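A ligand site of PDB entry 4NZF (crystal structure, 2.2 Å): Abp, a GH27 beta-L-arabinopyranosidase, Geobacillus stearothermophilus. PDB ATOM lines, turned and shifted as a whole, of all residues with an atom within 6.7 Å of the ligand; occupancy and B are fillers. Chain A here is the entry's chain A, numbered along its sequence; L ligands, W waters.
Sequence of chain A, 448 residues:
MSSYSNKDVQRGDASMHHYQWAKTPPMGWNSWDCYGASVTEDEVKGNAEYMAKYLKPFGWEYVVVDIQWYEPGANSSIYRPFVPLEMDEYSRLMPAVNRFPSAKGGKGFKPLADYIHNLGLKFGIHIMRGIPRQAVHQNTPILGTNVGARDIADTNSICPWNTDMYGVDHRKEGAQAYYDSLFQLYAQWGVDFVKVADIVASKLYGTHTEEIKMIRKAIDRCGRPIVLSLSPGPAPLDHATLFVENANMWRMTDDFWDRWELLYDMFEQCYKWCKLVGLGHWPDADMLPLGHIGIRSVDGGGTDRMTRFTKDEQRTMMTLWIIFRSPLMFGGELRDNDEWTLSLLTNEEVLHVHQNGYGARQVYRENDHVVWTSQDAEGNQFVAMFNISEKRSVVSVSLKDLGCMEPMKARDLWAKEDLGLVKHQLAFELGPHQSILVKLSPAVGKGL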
ATOM      1  N   ASN A  30      25.624   4.146 -13.501  1.00  0.00           N
ATOM      2  CA  ASN A  30      24.968   4.600 -12.341  1.00  0.00           C
ATOM      3  C   ASN A  30      25.928   5.455 -11.500  1.00  0.00           C
ATOM      4  O   ASN A  30      27.112   5.099 -11.305  1.00  0.00           O
ATOM      5  CB  ASN A  30      24.556   3.463 -11.543  1.00  0.00           C
ATOM      6  CG  ASN A  30      23.882   3.846 -10.284  1.00  0.00           C
ATOM      7  OD1 ASN A  30      24.481   4.366  -9.326  1.00  0.00           O
ATOM      8  ND2 ASN A  30      22.597   3.534 -10.231  1.00  0.00           N
ATOM      9  N   TRP A  32      26.310   6.204  -8.339  1.00  0.00           N
ATOM     10  CA  TRP A  32      26.562   6.008  -6.942  1.00  0.00           C
ATOM     11  C   TRP A  32      28.019   5.810  -6.587  1.00  0.00           C
ATOM     12  O   TRP A  32      28.552   6.412  -5.659  1.00  0.00           O
ATOM     13  CB  TRP A  32      25.787   4.807  -6.471  1.00  0.00           C
ATOM     14  CG  TRP A  32      26.062   4.367  -5.022  1.00  0.00           C
ATOM     15  CD1 TRP A  32      26.580   3.184  -4.662  1.00  0.00           C
ATOM     16  CD2 TRP A  32      25.703   5.032  -3.817  1.00  0.00           C
ATOM     17  NE1 TRP A  32      26.612   3.060  -3.289  1.00  0.00           N
ATOM     18  CE2 TRP A  32      26.102   4.202  -2.749  1.00  0.00           C
ATOM     19  CE3 TRP A  32      25.123   6.232  -3.526  1.00  0.00           C
ATOM     20  CZ2 TRP A  32      25.926   4.523  -1.466  1.00  0.00           C
ATOM     21  CZ3 TRP A  32      25.014   6.584  -2.252  1.00  0.00           C
ATOM     22  CH2 TRP A  32      25.372   5.724  -1.222  1.00  0.00           C
ATOM     23  N   ASP A  33      28.682   4.944  -7.329  1.00  0.00           N
ATOM     24  CA  ASP A  33      29.977   4.538  -6.914  1.00  0.00           C
ATOM     25  C   ASP A  33      30.934   5.696  -7.106  1.00  0.00           C
ATOM     26  O   ASP A  33      32.006   5.742  -6.441  1.00  0.00           O
ATOM     27  CB  ASP A  33      30.487   3.323  -7.720  1.00  0.00           C
ATOM     28  CG  ASP A  33      29.907   1.941  -7.251  1.00  0.00           C
ATOM     29  OD1 ASP A  33      29.103   1.855  -6.319  1.00  0.00           O
ATOM     30  OD2 ASP A  33      30.301   0.923  -7.853  1.00  0.00           O
ATOM     31  N   ASP A  66      21.533   8.209  -9.337  1.00  0.00           N
ATOM     32  CA  ASP A  66      21.267   7.441  -8.121  1.00  0.00           C
ATOM     33  C   ASP A  66      20.696   8.324  -6.988  1.00  0.00           C
ATOM     34  O   ASP A  66      20.138   9.419  -7.219  1.00  0.00           O
ATOM     35  CB  ASP A  66      22.504   6.656  -7.748  1.00  0.00           C
ATOM     36  CG  ASP A  66      22.166   5.366  -6.928  1.00  0.00           C
ATOM     37  OD1 ASP A  66      22.351   5.364  -5.690  1.00  0.00           O
ATOM     38  OD2 ASP A  66      21.694   4.403  -7.583  1.00  0.00           O
ATOM     39  N   ILE A  67      20.794   7.861  -5.753  1.00  0.00           N
ATOM     40  CA  ILE A  67      19.963   8.324  -4.687  1.00  0.00           C
ATOM     41  C   ILE A  67      20.119   9.852  -4.383  1.00  0.00           C
ATOM     42  O   ILE A  67      21.196  10.471  -4.570  1.00  0.00           O
ATOM     43  CB  ILE A  67      20.336   7.509  -3.449  1.00  0.00           C
ATOM     44  CG1 ILE A  67      19.447   7.830  -2.267  1.00  0.00           C
ATOM     45  CG2 ILE A  67      21.802   7.751  -3.103  1.00  0.00           C
ATOM     46  CD1 ILE A  67      19.508   6.796  -1.120  1.00  0.00           C
ATOM     47  N   TYR A  79      24.634  10.343   4.137  1.00  0.00           N
ATOM     48  CA  TYR A  79      23.480  11.158   3.962  1.00  0.00           C
ATOM     49  C   TYR A  79      23.522  12.202   5.151  1.00  0.00           C
ATOM     50  O   TYR A  79      23.995  11.880   6.259  1.00  0.00           O
ATOM     51  CB  TYR A  79      22.171  10.297   4.007  1.00  0.00           C
ATOM     52  CG  TYR A  79      22.178   9.146   3.099  1.00  0.00           C
ATOM     53  CD1 TYR A  79      22.257   9.348   1.707  1.00  0.00           C
ATOM     54  CD2 TYR A  79      22.284   7.873   3.587  1.00  0.00           C
ATOM     55  CE1 TYR A  79      22.383   8.310   0.833  1.00  0.00           C
ATOM     56  CE2 TYR A  79      22.411   6.782   2.720  1.00  0.00           C
ATOM     57  CZ  TYR A  79      22.454   6.992   1.355  1.00  0.00           C
ATOM     58  OH  TYR A  79      22.648   5.975   0.512  1.00  0.00           O
ATOM     59  N   HIS A 126      16.965   6.700  -9.200  1.00  0.00           N
ATOM     60  CA  HIS A 126      16.763   6.010  -7.947  1.00  0.00           C
ATOM     61  C   HIS A 126      15.664   6.663  -7.168  1.00  0.00           C
ATOM     62  O   HIS A 126      15.535   7.882  -7.218  1.00  0.00           O
ATOM     63  CB  HIS A 126      18.038   6.256  -7.171  1.00  0.00           C
ATOM     64  CG  HIS A 126      18.181   5.515  -5.908  1.00  0.00           C
ATOM     65  ND1 HIS A 126      17.470   5.797  -4.787  1.00  0.00           N
ATOM     66  CD2 HIS A 126      19.071   4.575  -5.548  1.00  0.00           C
ATOM     67  CE1 HIS A 126      17.879   5.058  -3.788  1.00  0.00           C
ATOM     68  NE2 HIS A 126      18.843   4.282  -4.238  1.00  0.00           N
ATOM     69  N   MET A 128      13.723   6.178  -3.125  1.00  0.00           N
ATOM     70  CA  MET A 128      13.629   5.528  -1.851  1.00  0.00           C
ATOM     71  C   MET A 128      12.213   5.070  -1.696  1.00  0.00           C
ATOM     72  O   MET A 128      11.322   5.835  -1.970  1.00  0.00           O
ATOM     73  CB  MET A 128      13.944   6.512  -0.711  1.00  0.00           C
ATOM     74  CG  MET A 128      15.432   6.848  -0.597  1.00  0.00           C
ATOM     75  SD  MET A 128      16.480   5.456  -0.156  1.00  0.00           S
ATOM     76  CE  MET A 128      15.895   4.850   1.401  1.00  0.00           C
ATOM     77  N   TRP A 161      18.983   3.084   7.437  1.00  0.00           N
ATOM     78  CA  TRP A 161      20.177   3.713   7.019  1.00  0.00           C
ATOM     79  C   TRP A 161      19.959   5.024   6.232  1.00  0.00           C
ATOM     80  O   TRP A 161      20.902   5.598   5.644  1.00  0.00           O
ATOM     81  CB  TRP A 161      20.990   2.712   6.191  1.00  0.00           C
ATOM     82  CG  TRP A 161      20.248   2.009   5.131  1.00  0.00           C
ATOM     83  CD1 TRP A 161      19.715   0.759   5.220  1.00  0.00           C
ATOM     84  CD2 TRP A 161      19.995   2.480   3.791  1.00  0.00           C
ATOM     85  NE1 TRP A 161      19.106   0.452   4.034  1.00  0.00           N
ATOM     86  CE2 TRP A 161      19.311   1.475   3.130  1.00  0.00           C
ATOM     87  CE3 TRP A 161      20.372   3.626   3.080  1.00  0.00           C
ATOM     88  CZ2 TRP A 161      18.874   1.604   1.800  1.00  0.00           C
ATOM     89  CZ3 TRP A 161      20.007   3.749   1.745  1.00  0.00           C
ATOM     90  CH2 TRP A 161      19.247   2.745   1.112  1.00  0.00           C
ATOM     91  N   LYS A 195      15.369   2.442 -10.031  1.00  0.00           N
ATOM     92  CA  LYS A 195      15.972   1.619  -9.009  1.00  0.00           C
ATOM     93  C   LYS A 195      15.376   2.023  -7.679  1.00  0.00           C
ATOM     94  O   LYS A 195      15.575   3.141  -7.257  1.00  0.00           O
ATOM     95  CB  LYS A 195      17.472   1.884  -9.061  1.00  0.00           C
ATOM     96  CG  LYS A 195      18.268   1.305  -7.906  1.00  0.00           C
ATOM     97  CD  LYS A 195      19.777   1.535  -8.080  1.00  0.00           C
ATOM     98  CE  LYS A 195      20.522   1.204  -6.796  1.00  0.00           C
ATOM     99  NZ  LYS A 195      21.998   1.445  -6.794  1.00  0.00           N
ATOM    100  N   VAL A 196      14.704   1.136  -7.002  1.00  0.00           N
ATOM    101  CA  VAL A 196      14.054   1.417  -5.762  1.00  0.00           C
ATOM    102  C   VAL A 196      14.950   0.872  -4.699  1.00  0.00           C
ATOM    103  O   VAL A 196      15.449  -0.274  -4.783  1.00  0.00           O
ATOM    104  CB  VAL A 196      12.743   0.727  -5.661  1.00  0.00           C
ATOM    105  CG1 VAL A 196      12.008   1.093  -4.381  1.00  0.00           C
ATOM    106  CG2 VAL A 196      11.915   0.992  -6.922  1.00  0.00           C
ATOM    107  N   ALA A 197      15.085   1.652  -3.633  1.00  0.00           N
ATOM    108  CA  ALA A 197      15.905   1.299  -2.476  1.00  0.00           C
ATOM    109  C   ALA A 197      15.118   1.069  -1.251  1.00  0.00           C
ATOM    110  O   ALA A 197      13.956   1.472  -1.184  1.00  0.00           O
ATOM    111  CB  ALA A 197      16.901   2.407  -2.255  1.00  0.00           C
ATOM    112  N   ASP A 198      15.731   0.465  -0.243  1.00  0.00           N
ATOM    113  CA  ASP A 198      15.063   0.097   1.040  1.00  0.00           C
ATOM    114  C   ASP A 198      13.814  -0.737   0.789  1.00  0.00           C
ATOM    115  O   ASP A 198      12.746  -0.562   1.453  1.00  0.00           O
ATOM    116  CB  ASP A 198      14.745   1.323   1.893  1.00  0.00           C
ATOM    117  CG  ASP A 198      14.108   0.985   3.205  1.00  0.00           C
ATOM    118  OD1 ASP A 198      14.629   0.116   3.936  1.00  0.00           O
ATOM    119  OD2 ASP A 198      13.052   1.597   3.584  1.00  0.00           O
ATOM    120  N   ILE A 199      13.999  -1.753  -0.033  1.00  0.00           N
ATOM    121  CA  ILE A 199      12.831  -2.543  -0.405  1.00  0.00           C
ATOM    122  C   ILE A 199      13.020  -4.050  -0.404  1.00  0.00           C
ATOM    123  O   ILE A 199      12.068  -4.740  -0.155  1.00  0.00           O
ATOM    124  CB  ILE A 199      12.184  -2.028  -1.734  1.00  0.00           C
ATOM    125  CG1 ILE A 199      10.734  -2.425  -1.807  1.00  0.00           C
ATOM    126  CG2 ILE A 199      12.918  -2.599  -2.926  1.00  0.00           C
ATOM    127  CD1 ILE A 199       9.805  -1.682  -2.730  1.00  0.00           C
ATOM    128  N   SER A 231      16.658  -2.936  -4.692  1.00  0.00           N
ATOM    129  CA  SER A 231      17.898  -2.826  -3.834  1.00  0.00           C
ATOM    130  C   SER A 231      17.559  -2.458  -2.383  1.00  0.00           C
ATOM    131  O   SER A 231      16.408  -2.099  -2.045  1.00  0.00           O
ATOM    132  CB  SER A 231      18.847  -1.756  -4.395  1.00  0.00           C
ATOM    133  OG  SER A 231      18.266  -0.475  -4.263  1.00  0.00           O
ATOM    134  N   PRO A 232      18.517  -2.615  -1.476  1.00  0.00           N
ATOM    135  CA  PRO A 232      19.735  -3.333  -1.607  1.00  0.00           C
ATOM    136  C   PRO A 232      19.462  -4.817  -1.304  1.00  0.00           C
ATOM    137  O   PRO A 232      18.423  -5.140  -0.794  1.00  0.00           O
ATOM    138  CB  PRO A 232      20.547  -2.726  -0.490  1.00  0.00           C
ATOM    139  CG  PRO A 232      19.571  -2.616   0.634  1.00  0.00           C
ATOM    140  CD  PRO A 232      18.349  -2.132  -0.086  1.00  0.00           C
ATOM    141  N   GLY A 233      20.421  -5.676  -1.560  1.00  0.00           N
ATOM    142  CA  GLY A 233      20.331  -7.071  -1.127  1.00  0.00           C
ATOM    143  C   GLY A 233      20.916  -7.212   0.285  1.00  0.00           C
ATOM    144  O   GLY A 233      21.292  -6.208   0.877  1.00  0.00           O
ATOM    145  N   ARG A 251      18.679  -7.103  -6.423  1.00  0.00           N
ATOM    146  CA  ARG A 251      20.061  -7.233  -5.878  1.00  0.00           C
ATOM    147  C   ARG A 251      20.234  -8.452  -5.023  1.00  0.00           C
ATOM    148  O   ARG A 251      19.558  -8.622  -4.060  1.00  0.00           O
ATOM    149  CB  ARG A 251      20.395  -5.967  -5.085  1.00  0.00           C
ATOM    150  CG  ARG A 251      20.760  -4.795  -6.046  1.00  0.00           C
ATOM    151  CD  ARG A 251      22.261  -4.663  -6.285  1.00  0.00           C
ATOM    152  NE  ARG A 251      22.803  -4.624  -4.956  1.00  0.00           N
ATOM    153  CZ  ARG A 251      22.862  -3.510  -4.219  1.00  0.00           C
ATOM    154  NH1 ARG A 251      22.672  -2.295  -4.784  1.00  0.00           N
ATOM    155  NH2 ARG A 251      23.239  -3.627  -2.958  1.00  0.00           N
ATOM    156  N   THR A 253      22.823  -9.012  -3.295  1.00  0.00           N
ATOM    157  CA  THR A 253      23.873  -8.722  -2.298  1.00  0.00           C
ATOM    158  C   THR A 253      23.701  -7.341  -1.733  1.00  0.00           C
ATOM    159  O   THR A 253      23.148  -6.466  -2.420  1.00  0.00           O
ATOM    160  CB  THR A 253      25.138  -8.846  -3.172  1.00  0.00           C
ATOM    161  OG1 THR A 253      25.760 -10.129  -3.001  1.00  0.00           O
ATOM    162  CG2 THR A 253      25.920  -7.828  -3.230  1.00  0.00           C
ATOM    163  N   ASP A 254      24.158  -7.105  -0.493  1.00  0.00           N
ATOM    164  CA  ASP A 254      24.326  -5.731   0.007  1.00  0.00           C
ATOM    165  C   ASP A 254      25.330  -5.046  -0.883  1.00  0.00           C
ATOM    166  O   ASP A 254      25.964  -5.715  -1.672  1.00  0.00           O
ATOM    167  CB  ASP A 254      24.851  -5.712   1.414  1.00  0.00           C
ATOM    168  CG  ASP A 254      24.599  -4.385   2.111  1.00  0.00           C
ATOM    169  OD1 ASP A 254      23.918  -3.491   1.585  1.00  0.00           O
ATOM    170  OD2 ASP A 254      25.084  -4.290   3.246  1.00  0.00           O
ATOM    171  N   ASP A 255      25.577  -3.749  -0.689  1.00  0.00           N
ATOM    172  CA  ASP A 255      26.295  -2.954  -1.698  1.00  0.00           C
ATOM    173  C   ASP A 255      27.654  -3.489  -2.082  1.00  0.00           C
ATOM    174  O   ASP A 255      28.464  -3.738  -1.227  1.00  0.00           O
ATOM    175  CB  ASP A 255      26.470  -1.474  -1.263  1.00  0.00           C
ATOM    176  CG  ASP A 255      25.114  -0.738  -1.040  1.00  0.00           C
ATOM    177  OD1 ASP A 255      24.036  -1.387  -1.176  1.00  0.00           O
ATOM    178  OD2 ASP A 255      25.123   0.480  -0.704  1.00  0.00           O
ATOM    179  N   PHE A 256      27.962  -3.556  -3.362  1.00  0.00           N
ATOM    180  CA  PHE A 256      29.184  -4.183  -3.789  1.00  0.00           C
ATOM    181  C   PHE A 256      30.236  -3.131  -4.020  1.00  0.00           C
ATOM    182  O   PHE A 256      29.915  -2.042  -4.505  1.00  0.00           O
ATOM    183  CB  PHE A 256      28.919  -5.058  -5.038  1.00  0.00           C
ATOM    184  CG  PHE A 256      30.145  -5.749  -5.634  1.00  0.00           C
ATOM    185  CD1 PHE A 256      30.593  -6.914  -5.130  1.00  0.00           C
ATOM    186  CD2 PHE A 256      30.733  -5.287  -6.721  1.00  0.00           C
ATOM    187  CE1 PHE A 256      31.734  -7.529  -5.646  1.00  0.00           C
ATOM    188  CE2 PHE A 256      31.834  -5.892  -7.287  1.00  0.00           C
ATOM    189  CZ  PHE A 256      32.300  -7.023  -6.751  1.00  0.00           C
ATOM    190  N   ASP A 286      24.965  -6.388  -8.827  1.00  0.00           N
ATOM    191  CA  ASP A 286      25.293  -4.955  -8.540  1.00  0.00           C
ATOM    192  C   ASP A 286      26.320  -4.350  -9.516  1.00  0.00           C
ATOM    193  O   ASP A 286      26.948  -4.984 -10.399  1.00  0.00           O
ATOM    194  CB  ASP A 286      25.689  -4.802  -7.058  1.00  0.00           C
ATOM    195  CG  ASP A 286      25.407  -3.362  -6.460  1.00  0.00           C
ATOM    196  OD1 ASP A 286      24.973  -2.421  -7.236  1.00  0.00           O
ATOM    197  OD2 ASP A 286      25.746  -3.199  -5.264  1.00  0.00           O
ATOM    198  N   MET A 287      26.469  -3.071  -9.323  1.00  0.00           N
ATOM    199  CA  MET A 287      27.228  -2.167 -10.128  1.00  0.00           C
ATOM    200  C   MET A 287      28.670  -2.538 -10.097  1.00  0.00           C
ATOM    201  O   MET A 287      29.123  -3.087  -9.178  1.00  0.00           O
ATOM    202  CB  MET A 287      26.995  -0.740  -9.560  1.00  0.00           C
ATOM    203  CG  MET A 287      25.542  -0.287  -9.670  1.00  0.00           C
ATOM    204  SD  MET A 287      25.167   1.223  -8.782  1.00  0.00           S
ATOM    205  CE  MET A 287      25.375   0.708  -7.064  1.00  0.00           C
HETATM  206  C1  LIG L   1      20.551   1.460  -2.374  1.00  0.00           C
HETATM  207  C2  LIG L   1      21.744   0.690  -3.008  1.00  0.00           C
HETATM  208  C3  LIG L   1      22.968   1.510  -3.300  1.00  0.00           C
HETATM  209  C4  LIG L   1      22.642   2.993  -3.476  1.00  0.00           C
HETATM  210  C5  LIG L   1      22.014   3.441  -2.203  1.00  0.00           C
HETATM  211  O1  LIG L   1      19.697   0.622  -1.519  1.00  0.00           O
HETATM  212  O2  LIG L   1      22.043  -0.539  -2.414  1.00  0.00           O
HETATM  213  O3  LIG L   1      23.457   0.986  -4.523  1.00  0.00           O
HETATM  214  O4  LIG L   1      21.677   3.313  -4.453  1.00  0.00           O
HETATM  215  O5  LIG L   1      20.795   2.786  -1.820  1.00  0.00           O
HETATM  216  O   HOH W   1      25.426  -0.654  -4.233  1.00  0.00           O
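Water W1 lies within hydrogen-bond range of O3 of the ligand (2.6 Å), OD2 of Asp 286 (2.8 Å), NH1 of Arg 251 (3.3 Å) and OD1 of Asp 255 (3.4 Å).
The side-chain carboxylate (OD1) of Asp 66 lies within hydrogen-bond range of an oxygen (O4) of the ligand, at 2.5 Å. An oxygen (O2) of the ligand lies within hydrogen-bond range of the side-chain carboxylate of Asp 255. NZ of Lys 195 lies within hydrogen-bond range of O3 of the ligand (2.7 Å). An oxygen (O4) of the ligand is in hydrogen-bond range of a ring nitrogen (NE2) of His 126, at 3.0 Å. An oxygen (O2) of the ligand is in hydrogen-bond range of the guanidinium group (NH1) of Arg 251, 3.0 Å away. An oxygen (O1) of the ligand is in hydrogen-bond range of the side-chain hydroxyl (OG) of Ser 231 (3.3 Å).
NZ of Lys 195 is in salt-bridge range of OD2 of Asp 66 (3.1 Å). ND2 of Asn 30 sits at hydrogen-bond distance from OD2 of Asp 66 (2.9 Å). The side-chain carboxylate (OD1) of Asp 255 is in salt-bridge range of the guanidinium group (NH2) of Arg 251, at 3.0 Å. The side-chain sulfur of Met 287 sits close to the side-chain amino group of Lys 195 (3.7 Å). The side-chain amide oxygen (OD1) of Asn 30 sits close to the side-chain sulfur (SD) of Met 287 (3.3 Å). OG of Ser 231 sits at hydrogen-bond distance from O of Val 196 (2.9 Å). The backbone NH (N) of Ile 199 is in hydrogen-bond range of the backbone carbonyl oxygen (O) of Ser 231 (3.2 Å). The side-chain amide oxygen (OD1) of Asn 30 is in hydrogen-bond range of the backbone NH (N) of Trp 32.
An oxygen (O1) of the ligand sits close to the backbone nitrogen of Pro 232. Residues that only touch the ligand: Met 287, Trp 161, Ala 197, Trp 32 and Tyr 79. 12 residues have an atom within 4 Å of the ligand: Trp 32, Asp 66, Tyr 79, His 126, Trp 161, Lys 195, Ala 197, Ser 231, Pro 232, Arg 251, Asp 255 and Met 287.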
